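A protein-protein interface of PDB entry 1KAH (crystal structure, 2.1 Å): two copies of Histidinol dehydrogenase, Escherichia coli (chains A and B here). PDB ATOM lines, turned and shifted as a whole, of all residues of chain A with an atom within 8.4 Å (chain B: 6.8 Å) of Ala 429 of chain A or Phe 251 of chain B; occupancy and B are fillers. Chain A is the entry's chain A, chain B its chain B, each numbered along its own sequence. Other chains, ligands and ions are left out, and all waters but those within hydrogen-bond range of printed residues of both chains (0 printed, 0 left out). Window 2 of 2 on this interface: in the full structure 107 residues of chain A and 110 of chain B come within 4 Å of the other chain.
The guanidinium group of Arg 426 of chain A lies within hydrogen-bond range of the side-chain hydroxyl of Ser 254 of chain B (3.3 Å).
The side-chain carboxylate (OD2) of Asp 255 of chain B is in salt-bridge range of the guanidinium group (NH2) of Arg 426 of chain A, 2.7 Å away.
NE of Arg 426 of chain A lies within hydrogen-bond range of O of Asp 352 of chain B (2.6 Å).
The backbone carbonyl oxygen (O) of Ala 422 of chain A sits at hydrogen-bond distance from the guanidinium group (NH1) of Arg 426 of chain A (3.0 Å).
The side-chain hydroxyl of Ser 254 of chain B sits at hydrogen-bond distance from the backbone carbonyl oxygen of Asp 250 of chain B.
The side-chain amide nitrogen (NE2) of Gln 288 of chain B lies within hydrogen-bond range of the side-chain carboxylate (OD1) of Asp 250 of chain B, at 2.8 Å.
The side-chain hydroxyl (OG) of Ser 254 of chain B is in hydrogen-bond range of the backbone carbonyl oxygen (O) of Phe 251 of chain B (2.8 Å).
The backbone NH of Ser 254 of chain B sits close to the side-chain amide oxygen of Gln 288 of chain B (3.5 Å).
OD2 of Asp 255 of chain B is in hydrogen-bond range of NE2 of Gln 331 of chain B, at 2.9 Å.
Among the printed residues, pairs that only touch across the chains: Lys 397 of chain A with Trp 353 of chain B, Phe 400 of chain A with Trp 353 of chain B, Ala 422 of chain A with Ser 254 of chain B, Leu 425 of chain A with Asp 250 of chain B, Leu 425 of chain A with Phe 251 of chain B, Leu 425 of chain A with Ser 254 of chain B, Leu 425 of chain A with Gln 288 of chain B, Arg 426 of chain A with Phe 251 of chain B, Arg 426 of chain A with Gln 331 of chain B, Arg 426 of chain A with Trp 353 of chain B, Ala 429 of chain A with Phe 251 of chain B and Leu 430 of chain A with Trp 353 of chain B.
Ala 429 of chain A touches just one residue of chain B: Phe 251.
Of the printed residues of chain B, Phe 400 of chain A touches Trp 353.
Printed residues of chain A within 4 Å of Gln 331 of chain B: Arg 426.
Of the printed residues of chain A, Asp 250 of chain B touches Leu 425.
Printed residues of chain A within 4 Å of Ser 254 of chain B: Ala 422 (3.6 Å), Leu 425 (3.6 Å) and Arg 426 (3.3 Å).
Of the printed residues of chain A, Gln 288 of chain B touches Leu 425.
Ala 253 of chain B touches none of the printed residues of chain A.
The nearest residue of chain B that does not touch Ala 429 of chain A is Trp 353 of chain B (4.5 Å).
Hydrophobic or aromatic side chains of chain A that line the printed part of chain B: Phe 400, Ala 422, Leu 425, Ala 429 and Leu 430.
Of the 17 printed residues of chain B, 8 touch a printed residue of chain A.
Hydrophobic or aromatic side chains of chain B that line the printed part of chain A: Phe 251 and Trp 353.
Among the printed residues, 15 pairs touch across the chains.
No position is printed for both chains.
Of the 15 pairs that touch across the chains among the printed residues, none has its exchanged pair printed and touching as well.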
ATOM      1  N   LYS A 397      -7.078  19.687   9.300  1.00  0.00           N
ATOM      2  CA  LYS A 397      -7.930  19.213  10.378  1.00  0.00           C
ATOM      3  C   LYS A 397      -9.250  18.731   9.797  1.00  0.00           C
ATOM      4  O   LYS A 397      -9.774  17.692  10.195  1.00  0.00           O
ATOM      5  CB  LYS A 397      -8.191  20.329  11.391  1.00  0.00           C
ATOM      6  CG  LYS A 397      -6.959  20.772  12.164  1.00  0.00           C
ATOM      7  CD  LYS A 397      -7.324  21.825  13.197  1.00  0.00           C
ATOM      8  CE  LYS A 397      -6.102  22.328  13.936  1.00  0.00           C
ATOM      9  NZ  LYS A 397      -6.411  23.528  14.777  1.00  0.00           N
ATOM     10  N   PHE A 400      -8.641  15.397   7.664  1.00  0.00           N
ATOM     11  CA  PHE A 400      -8.426  14.259   8.555  1.00  0.00           C
ATOM     12  C   PHE A 400      -9.730  13.827   9.226  1.00  0.00           C
ATOM     13  O   PHE A 400     -10.050  12.642   9.240  1.00  0.00           O
ATOM     14  CB  PHE A 400      -7.368  14.575   9.629  1.00  0.00           C
ATOM     15  CG  PHE A 400      -7.366  13.595  10.781  1.00  0.00           C
ATOM     16  CD1 PHE A 400      -8.092  13.863  11.936  1.00  0.00           C
ATOM     17  CD2 PHE A 400      -6.697  12.374  10.680  1.00  0.00           C
ATOM     18  CE1 PHE A 400      -8.162  12.931  12.978  1.00  0.00           C
ATOM     19  CE2 PHE A 400      -6.762  11.434  11.717  1.00  0.00           C
ATOM     20  CZ  PHE A 400      -7.498  11.715  12.869  1.00  0.00           C
ATOM     21  N   ALA A 418      -2.750  -0.172  17.176  1.00  0.00           N
ATOM     22  CA  ALA A 418      -1.971   1.062  17.227  1.00  0.00           C
ATOM     23  C   ALA A 418      -2.323   1.959  16.047  1.00  0.00           C
ATOM     24  O   ALA A 418      -2.361   3.183  16.175  1.00  0.00           O
ATOM     25  CB  ALA A 418      -0.464   0.755  17.223  1.00  0.00           C
ATOM     26  N   ASN A 421      -5.599   3.464  17.096  1.00  0.00           N
ATOM     27  CA  ASN A 421      -5.428   4.424  18.181  1.00  0.00           C
ATOM     28  C   ASN A 421      -4.778   5.729  17.751  1.00  0.00           C
ATOM     29  O   ASN A 421      -4.974   6.749  18.403  1.00  0.00           O
ATOM     30  CB  ASN A 421      -4.602   3.839  19.331  1.00  0.00           C
ATOM     31  CG  ASN A 421      -5.282   2.667  20.009  1.00  0.00           C
ATOM     32  OD1 ASN A 421      -6.481   2.435  19.839  1.00  0.00           O
ATOM     33  ND2 ASN A 421      -4.515   1.924  20.799  1.00  0.00           N
ATOM     34  N   ALA A 422      -3.995   5.706  16.676  1.00  0.00           N
ATOM     35  CA  ALA A 422      -3.344   6.920  16.197  1.00  0.00           C
ATOM     36  C   ALA A 422      -4.405   7.875  15.668  1.00  0.00           C
ATOM     37  O   ALA A 422      -4.201   9.085  15.635  1.00  0.00           O
ATOM     38  CB  ALA A 422      -2.342   6.591  15.089  1.00  0.00           C
ATOM     39  N   VAL A 423      -5.530   7.323  15.236  1.00  0.00           N
ATOM     40  CA  VAL A 423      -6.623   8.135  14.719  1.00  0.00           C
ATOM     41  C   VAL A 423      -7.491   8.645  15.868  1.00  0.00           C
ATOM     42  O   VAL A 423      -7.844   9.824  15.918  1.00  0.00           O
ATOM     43  CB  VAL A 423      -7.509   7.321  13.742  1.00  0.00           C
ATOM     44  CG1 VAL A 423      -8.702   8.169  13.285  1.00  0.00           C
ATOM     45  CG2 VAL A 423      -6.667   6.867  12.539  1.00  0.00           C
ATOM     46  N   THR A 424      -7.826   7.750  16.791  1.00  0.00           N
ATOM     47  CA  THR A 424      -8.651   8.101  17.937  1.00  0.00           C
ATOM     48  C   THR A 424      -8.014   9.210  18.763  1.00  0.00           C
ATOM     49  O   THR A 424      -8.706  10.131  19.214  1.00  0.00           O
ATOM     50  CB  THR A 424      -8.877   6.882  18.825  1.00  0.00           C
ATOM     51  OG1 THR A 424      -9.409   5.823  18.027  1.00  0.00           O
ATOM     52  CG2 THR A 424      -9.855   7.208  19.947  1.00  0.00           C
ATOM     53  N   LEU A 425      -6.701   9.125  18.974  1.00  0.00           N
ATOM     54  CA  LEU A 425      -6.007  10.157  19.734  1.00  0.00           C
ATOM     55  C   LEU A 425      -6.211  11.515  19.064  1.00  0.00           C
ATOM     56  O   LEU A 425      -6.516  12.515  19.721  1.00  0.00           O
ATOM     57  CB  LEU A 425      -4.512   9.853  19.822  1.00  0.00           C
ATOM     58  CG  LEU A 425      -4.141   8.763  20.833  1.00  0.00           C
ATOM     59  CD1 LEU A 425      -2.685   8.351  20.624  1.00  0.00           C
ATOM     60  CD2 LEU A 425      -4.364   9.288  22.266  1.00  0.00           C
ATOM     61  N   ARG A 426      -6.050  11.548  17.748  1.00  0.00           N
ATOM     62  CA  ARG A 426      -6.218  12.794  17.019  1.00  0.00           C
ATOM     63  C   ARG A 426      -7.671  13.270  16.983  1.00  0.00           C
ATOM     64  O   ARG A 426      -7.934  14.462  17.135  1.00  0.00           O
ATOM     65  CB  ARG A 426      -5.650  12.635  15.611  1.00  0.00           C
ATOM     66  CG  ARG A 426      -4.125  12.595  15.591  1.00  0.00           C
ATOM     67  CD  ARG A 426      -3.640  12.205  14.205  1.00  0.00           C
ATOM     68  NE  ARG A 426      -2.210  12.364  13.977  1.00  0.00           N
ATOM     69  CZ  ARG A 426      -1.268  11.506  14.363  1.00  0.00           C
ATOM     70  NH1 ARG A 426      -1.587  10.409  15.028  1.00  0.00           N
ATOM     71  NH2 ARG A 426      -0.002  11.716  14.019  1.00  0.00           N
ATOM     72  N   VAL A 427      -8.614  12.352  16.810  1.00  0.00           N
ATOM     73  CA  VAL A 427     -10.017  12.751  16.789  1.00  0.00           C
ATOM     74  C   VAL A 427     -10.417  13.327  18.154  1.00  0.00           C
ATOM     75  O   VAL A 427     -11.145  14.315  18.219  1.00  0.00           O
ATOM     76  CB  VAL A 427     -10.955  11.577  16.461  1.00  0.00           C
ATOM     77  CG1 VAL A 427     -12.413  12.043  16.531  1.00  0.00           C
ATOM     78  CG2 VAL A 427     -10.676  11.056  15.069  1.00  0.00           C
ATOM     79  N   ASN A 428      -9.937  12.729  19.241  1.00  0.00           N
ATOM     80  CA  ASN A 428     -10.298  13.237  20.561  1.00  0.00           C
ATOM     81  C   ASN A 428      -9.694  14.611  20.833  1.00  0.00           C
ATOM     82  O   ASN A 428     -10.326  15.446  21.478  1.00  0.00           O
ATOM     83  CB  ASN A 428      -9.872  12.267  21.668  1.00  0.00           C
ATOM     84  CG  ASN A 428     -10.688  10.994  21.671  1.00  0.00           C
ATOM     85  OD1 ASN A 428     -11.828  10.985  21.230  1.00  0.00           O
ATOM     86  ND2 ASN A 428     -10.111   9.917  22.179  1.00  0.00           N
ATOM     87  N   ALA A 429      -8.479  14.841  20.344  1.00  0.00           N
ATOM     88  CA  ALA A 429      -7.801  16.116  20.538  1.00  0.00           C
ATOM     89  C   ALA A 429      -8.591  17.201  19.820  1.00  0.00           C
ATOM     90  O   ALA A 429      -8.803  18.292  20.364  1.00  0.00           O
ATOM     91  CB  ALA A 429      -6.390  16.053  19.986  1.00  0.00           C
ATOM     92  N   LEU A 430      -9.015  16.905  18.595  1.00  0.00           N
ATOM     93  CA  LEU A 430      -9.792  17.866  17.825  1.00  0.00           C
ATOM     94  C   LEU A 430     -11.129  18.163  18.509  1.00  0.00           C
ATOM     95  O   LEU A 430     -11.561  19.309  18.552  1.00  0.00           O
ATOM     96  CB  LEU A 430     -10.024  17.353  16.396  1.00  0.00           C
ATOM     97  CG  LEU A 430      -8.779  17.438  15.501  1.00  0.00           C
ATOM     98  CD1 LEU A 430      -9.061  16.818  14.136  1.00  0.00           C
ATOM     99  CD2 LEU A 430      -8.353  18.908  15.354  1.00  0.00           C
ATOM    100  N   LYS A 431     -11.776  17.137  19.056  1.00  0.00           N
ATOM    101  CA  LYS A 431     -13.050  17.339  19.741  1.00  0.00           C
ATOM    102  C   LYS A 431     -12.915  18.302  20.915  1.00  0.00           C
ATOM    103  O   LYS A 431     -13.817  19.079  21.187  1.00  0.00           O
ATOM    104  CB  LYS A 431     -13.616  16.017  20.270  1.00  0.00           C
ATOM    105  CG  LYS A 431     -14.134  15.077  19.215  1.00  0.00           C
ATOM    106  CD  LYS A 431     -14.897  13.901  19.843  1.00  0.00           C
ATOM    107  CE  LYS A 431     -15.340  12.914  18.768  1.00  0.00           C
ATOM    108  NZ  LYS A 431     -16.085  11.763  19.338  1.00  0.00           N
ATOM    109  N   GLU A 432     -11.798  18.234  21.626  1.00  0.00           N
ATOM    110  CA  GLU A 432     -11.593  19.115  22.766  1.00  0.00           C
ATOM    111  C   GLU A 432     -11.226  20.544  22.398  1.00  0.00           C
ATOM    112  O   GLU A 432     -11.352  21.438  23.227  1.00  0.00           O
ATOM    113  CB  GLU A 432     -10.517  18.559  23.685  1.00  0.00           C
ATOM    114  CG  GLU A 432     -10.979  17.408  24.524  1.00  0.00           C
ATOM    115  CD  GLU A 432     -10.037  17.153  25.673  1.00  0.00           C
ATOM    116  OE1 GLU A 432     -10.084  17.920  26.673  1.00  0.00           O
ATOM    117  OE2 GLU A 432      -9.235  16.195  25.567  1.00  0.00           O
ATOM    118  N   GLN A 433     -10.767  20.754  21.168  1.00  0.00           N
ATOM    119  CA  GLN A 433     -10.388  22.086  20.702  1.00  0.00           C
ATOM    120  C   GLN A 433     -11.489  22.729  19.877  1.00  0.00           C
ATOM    121  O   GLN A 433     -11.435  23.922  19.576  1.00  0.00           O
ATOM    122  CB  GLN A 433      -9.160  22.001  19.821  1.00  0.00           C
ATOM    123  CG  GLN A 433      -7.863  21.739  20.513  1.00  0.00           C
ATOM    124  CD  GLN A 433      -6.784  21.390  19.506  1.00  0.00           C
ATOM    125  OE1 GLN A 433      -6.832  21.831  18.352  1.00  0.00           O
ATOM    126  NE2 GLN A 433      -5.808  20.596  19.931  1.00  0.00           N
ATOM    127  N   ALA A 434     -12.469  21.920  19.492  1.00  0.00           N
ATOM    128  CA  ALA A 434     -13.582  22.360  18.671  1.00  0.00           C
ATOM    129  C   ALA A 434     -14.463  23.408  19.340  1.00  0.00           C
ATOM    130  O   ALA A 434     -15.033  24.239  18.601  1.00  0.00           O
ATOM    131  CB  ALA A 434     -14.420  21.156  18.259  1.00  0.00           C
ATOM    132  OXT ALA A 434     -14.589  23.377  20.581  1.00  0.00           O
ATOM    133  N   VAL B 241      10.385   9.956  12.483  1.00  0.00           N
ATOM    134  CA  VAL B 241       9.579  11.130  12.772  1.00  0.00           C
ATOM    135  C   VAL B 241      10.469  12.288  13.162  1.00  0.00           C
ATOM    136  O   VAL B 241      11.359  12.131  13.992  1.00  0.00           O
ATOM    137  CB  VAL B 241       8.599  10.875  13.942  1.00  0.00           C
ATOM    138  CG1 VAL B 241       7.756  12.129  14.192  1.00  0.00           C
ATOM    139  CG2 VAL B 241       7.718   9.658  13.645  1.00  0.00           C
ATOM    140  N   ALA B 247       5.319  19.626  18.752  1.00  0.00           N
ATOM    141  CA  ALA B 247       4.615  18.370  18.540  1.00  0.00           C
ATOM    142  C   ALA B 247       3.945  17.842  19.801  1.00  0.00           C
ATOM    143  O   ALA B 247       4.304  18.212  20.922  1.00  0.00           O
ATOM    144  CB  ALA B 247       5.567  17.321  17.991  1.00  0.00           C
ATOM    145  N   THR B 248       2.972  16.962  19.605  1.00  0.00           N
ATOM    146  CA  THR B 248       2.236  16.345  20.706  1.00  0.00           C
ATOM    147  C   THR B 248       2.865  14.971  20.948  1.00  0.00           C
ATOM    148  O   THR B 248       2.876  14.127  20.058  1.00  0.00           O
ATOM    149  CB  THR B 248       0.734  16.201  20.333  1.00  0.00           C
ATOM    150  OG1 THR B 248       0.189  17.504  20.089  1.00  0.00           O
ATOM    151  CG2 THR B 248      -0.043  15.544  21.444  1.00  0.00           C
ATOM    152  N   PRO B 249       3.416  14.741  22.153  1.00  0.00           N
ATOM    153  CA  PRO B 249       4.050  13.458  22.472  1.00  0.00           C
ATOM    154  C   PRO B 249       3.224  12.246  22.085  1.00  0.00           C
ATOM    155  O   PRO B 249       3.750  11.289  21.514  1.00  0.00           O
ATOM    156  CB  PRO B 249       4.280  13.553  23.979  1.00  0.00           C
ATOM    157  CG  PRO B 249       4.570  15.012  24.173  1.00  0.00           C
ATOM    158  CD  PRO B 249       3.524  15.680  23.288  1.00  0.00           C
ATOM    159  N   ASP B 250       1.929  12.285  22.391  1.00  0.00           N
ATOM    160  CA  ASP B 250       1.046  11.173  22.083  1.00  0.00           C
ATOM    161  C   ASP B 250       0.869  10.913  20.601  1.00  0.00           C
ATOM    162  O   ASP B 250       0.686   9.764  20.189  1.00  0.00           O
ATOM    163  CB  ASP B 250      -0.325  11.361  22.745  1.00  0.00           C
ATOM    164  CG  ASP B 250      -0.342  10.887  24.187  1.00  0.00           C
ATOM    165  OD1 ASP B 250       0.166   9.775  24.458  1.00  0.00           O
ATOM    166  OD2 ASP B 250      -0.872  11.619  25.051  1.00  0.00           O
ATOM    167  N   PHE B 251       0.908  11.968  19.800  1.00  0.00           N
ATOM    168  CA  PHE B 251       0.774  11.810  18.349  1.00  0.00           C
ATOM    169  C   PHE B 251       2.048  11.137  17.835  1.00  0.00           C
ATOM    170  O   PHE B 251       1.999  10.201  17.029  1.00  0.00           O
ATOM    171  CB  PHE B 251       0.627  13.177  17.659  1.00  0.00           C
ATOM    172  CG  PHE B 251      -0.710  13.849  17.877  1.00  0.00           C
ATOM    173  CD1 PHE B 251      -1.717  13.231  18.610  1.00  0.00           C
ATOM    174  CD2 PHE B 251      -0.953  15.105  17.340  1.00  0.00           C
ATOM    175  CE1 PHE B 251      -2.956  13.859  18.808  1.00  0.00           C
ATOM    176  CE2 PHE B 251      -2.188  15.748  17.529  1.00  0.00           C
ATOM    177  CZ  PHE B 251      -3.191  15.120  18.266  1.00  0.00           C
ATOM    178  N   VAL B 252       3.192  11.630  18.302  1.00  0.00           N
ATOM    179  CA  VAL B 252       4.479  11.086  17.892  1.00  0.00           C
ATOM    180  C   VAL B 252       4.524   9.619  18.251  1.00  0.00           C
ATOM    181  O   VAL B 252       4.818   8.763  17.408  1.00  0.00           O
ATOM    182  CB  VAL B 252       5.662  11.786  18.611  1.00  0.00           C
ATOM    183  CG1 VAL B 252       6.993  11.208  18.112  1.00  0.00           C
ATOM    184  CG2 VAL B 252       5.616  13.275  18.360  1.00  0.00           C
ATOM    185  N   ALA B 253       4.228   9.337  19.517  1.00  0.00           N
ATOM    186  CA  ALA B 253       4.246   7.973  20.026  1.00  0.00           C
ATOM    187  C   ALA B 253       3.287   7.046  19.277  1.00  0.00           C
ATOM    188  O   ALA B 253       3.638   5.900  18.975  1.00  0.00           O
ATOM    189  CB  ALA B 253       3.935   7.967  21.529  1.00  0.00           C
ATOM    190  N   SER B 254       2.088   7.525  18.960  1.00  0.00           N
ATOM    191  CA  SER B 254       1.142   6.671  18.256  1.00  0.00           C
ATOM    192  C   SER B 254       1.665   6.310  16.864  1.00  0.00           C
ATOM    193  O   SER B 254       1.361   5.231  16.320  1.00  0.00           O
ATOM    194  CB  SER B 254      -0.232   7.346  18.156  1.00  0.00           C
ATOM    195  OG  SER B 254      -0.208   8.483  17.303  1.00  0.00           O
ATOM    196  N   ASP B 255       2.460   7.191  16.275  1.00  0.00           N
ATOM    197  CA  ASP B 255       3.000   6.882  14.954  1.00  0.00           C
ATOM    198  C   ASP B 255       4.151   5.880  15.047  1.00  0.00           C
ATOM    199  O   ASP B 255       4.284   5.003  14.200  1.00  0.00           O
ATOM    200  CB  ASP B 255       3.438   8.153  14.243  1.00  0.00           C
ATOM    201  CG  ASP B 255       2.252   8.965  13.744  1.00  0.00           C
ATOM    202  OD1 ASP B 255       1.387   8.376  13.047  1.00  0.00           O
ATOM    203  OD2 ASP B 255       2.187  10.178  14.039  1.00  0.00           O
ATOM    204  N   LEU B 256       4.970   5.999  16.087  1.00  0.00           N
ATOM    205  CA  LEU B 256       6.088   5.079  16.278  1.00  0.00           C
ATOM    206  C   LEU B 256       5.539   3.678  16.533  1.00  0.00           C
ATOM    207  O   LEU B 256       6.100   2.705  16.042  1.00  0.00           O
ATOM    208  CB  LEU B 256       6.955   5.513  17.466  1.00  0.00           C
ATOM    209  CG  LEU B 256       7.691   6.845  17.307  1.00  0.00           C
ATOM    210  CD1 LEU B 256       8.346   7.230  18.632  1.00  0.00           C
ATOM    211  CD2 LEU B 256       8.744   6.722  16.190  1.00  0.00           C
ATOM    212  N   ALA B 284       5.331   8.392  26.653  1.00  0.00           N
ATOM    213  CA  ALA B 284       4.044   8.191  25.994  1.00  0.00           C
ATOM    214  C   ALA B 284       4.058   6.824  25.324  1.00  0.00           C
ATOM    215  O   ALA B 284       3.069   6.087  25.350  1.00  0.00           O
ATOM    216  CB  ALA B 284       3.800   9.272  24.961  1.00  0.00           C
ATOM    217  N   GLN B 288       1.332   4.007  26.105  1.00  0.00           N
ATOM    218  CA  GLN B 288       0.451   3.489  25.060  1.00  0.00           C
ATOM    219  C   GLN B 288       0.700   2.011  24.823  1.00  0.00           C
ATOM    220  O   GLN B 288      -0.229   1.241  24.592  1.00  0.00           O
ATOM    221  CB  GLN B 288       0.641   4.269  23.755  1.00  0.00           C
ATOM    222  CG  GLN B 288       0.061   5.679  23.780  1.00  0.00           C
ATOM    223  CD  GLN B 288       0.303   6.433  22.475  1.00  0.00           C
ATOM    224  OE1 GLN B 288       0.244   5.857  21.392  1.00  0.00           O
ATOM    225  NE2 GLN B 288       0.566   7.726  22.581  1.00  0.00           N
ATOM    226  N   GLN B 331       6.485  16.398  12.046  1.00  0.00           N
ATOM    227  CA  GLN B 331       5.625  17.085  12.995  1.00  0.00           C
ATOM    228  C   GLN B 331       6.340  18.301  13.584  1.00  0.00           C
ATOM    229  O   GLN B 331       6.710  18.322  14.753  1.00  0.00           O
ATOM    230  CB  GLN B 331       5.168  16.109  14.092  1.00  0.00           C
ATOM    231  CG  GLN B 331       4.160  15.083  13.584  1.00  0.00           C
ATOM    232  CD  GLN B 331       3.768  14.044  14.623  1.00  0.00           C
ATOM    233  OE1 GLN B 331       3.849  14.283  15.823  1.00  0.00           O
ATOM    234  NE2 GLN B 331       3.324  12.883  14.157  1.00  0.00           N
ATOM    235  N   GLY B 351       2.551  17.576   9.226  1.00  0.00           N
ATOM    236  CA  GLY B 351       1.677  18.077  10.277  1.00  0.00           C
ATOM    237  C   GLY B 351       1.135  17.062  11.261  1.00  0.00           C
ATOM    238  O   GLY B 351       1.342  15.849  11.125  1.00  0.00           O
ATOM    239  N   ASP B 352       0.425  17.573  12.257  1.00  0.00           N
ATOM    240  CA  ASP B 352      -0.168  16.752  13.301  1.00  0.00           C
ATOM    241  C   ASP B 352      -1.335  15.873  12.864  1.00  0.00           C
ATOM    242  O   ASP B 352      -1.655  14.901  13.542  1.00  0.00           O
ATOM    243  CB  ASP B 352      -0.674  17.632  14.451  1.00  0.00           C
ATOM    244  CG  ASP B 352       0.443  18.322  15.220  1.00  0.00           C
ATOM    245  OD1 ASP B 352       1.452  17.669  15.574  1.00  0.00           O
ATOM    246  OD2 ASP B 352       0.288  19.526  15.499  1.00  0.00           O
ATOM    247  N   TRP B 353      -1.987  16.209  11.757  1.00  0.00           N
ATOM    248  CA  TRP B 353      -3.150  15.443  11.329  1.00  0.00           C
ATOM    249  C   TRP B 353      -2.925  14.480  10.176  1.00  0.00           C
ATOM    250  O   TRP B 353      -3.886  14.044   9.527  1.00  0.00           O
ATOM    251  CB  TRP B 353      -4.290  16.411  10.994  1.00  0.00           C
ATOM    252  CG  TRP B 353      -4.334  17.534  11.975  1.00  0.00           C
ATOM    253  CD1 TRP B 353      -3.910  18.808  11.767  1.00  0.00           C
ATOM    254  CD2 TRP B 353      -4.640  17.434  13.374  1.00  0.00           C
ATOM    255  NE1 TRP B 353      -3.914  19.505  12.950  1.00  0.00           N
ATOM    256  CE2 TRP B 353      -4.356  18.684  13.953  1.00  0.00           C
ATOM    257  CE3 TRP B 353      -5.119  16.404  14.194  1.00  0.00           C
ATOM    258  CZ2 TRP B 353      -4.530  18.938  15.316  1.00  0.00           C
ATOM    259  CZ3 TRP B 353      -5.296  16.652  15.545  1.00  0.00           C
ATOM    260  CH2 TRP B 353      -5.000  17.909  16.094  1.00  0.00           C
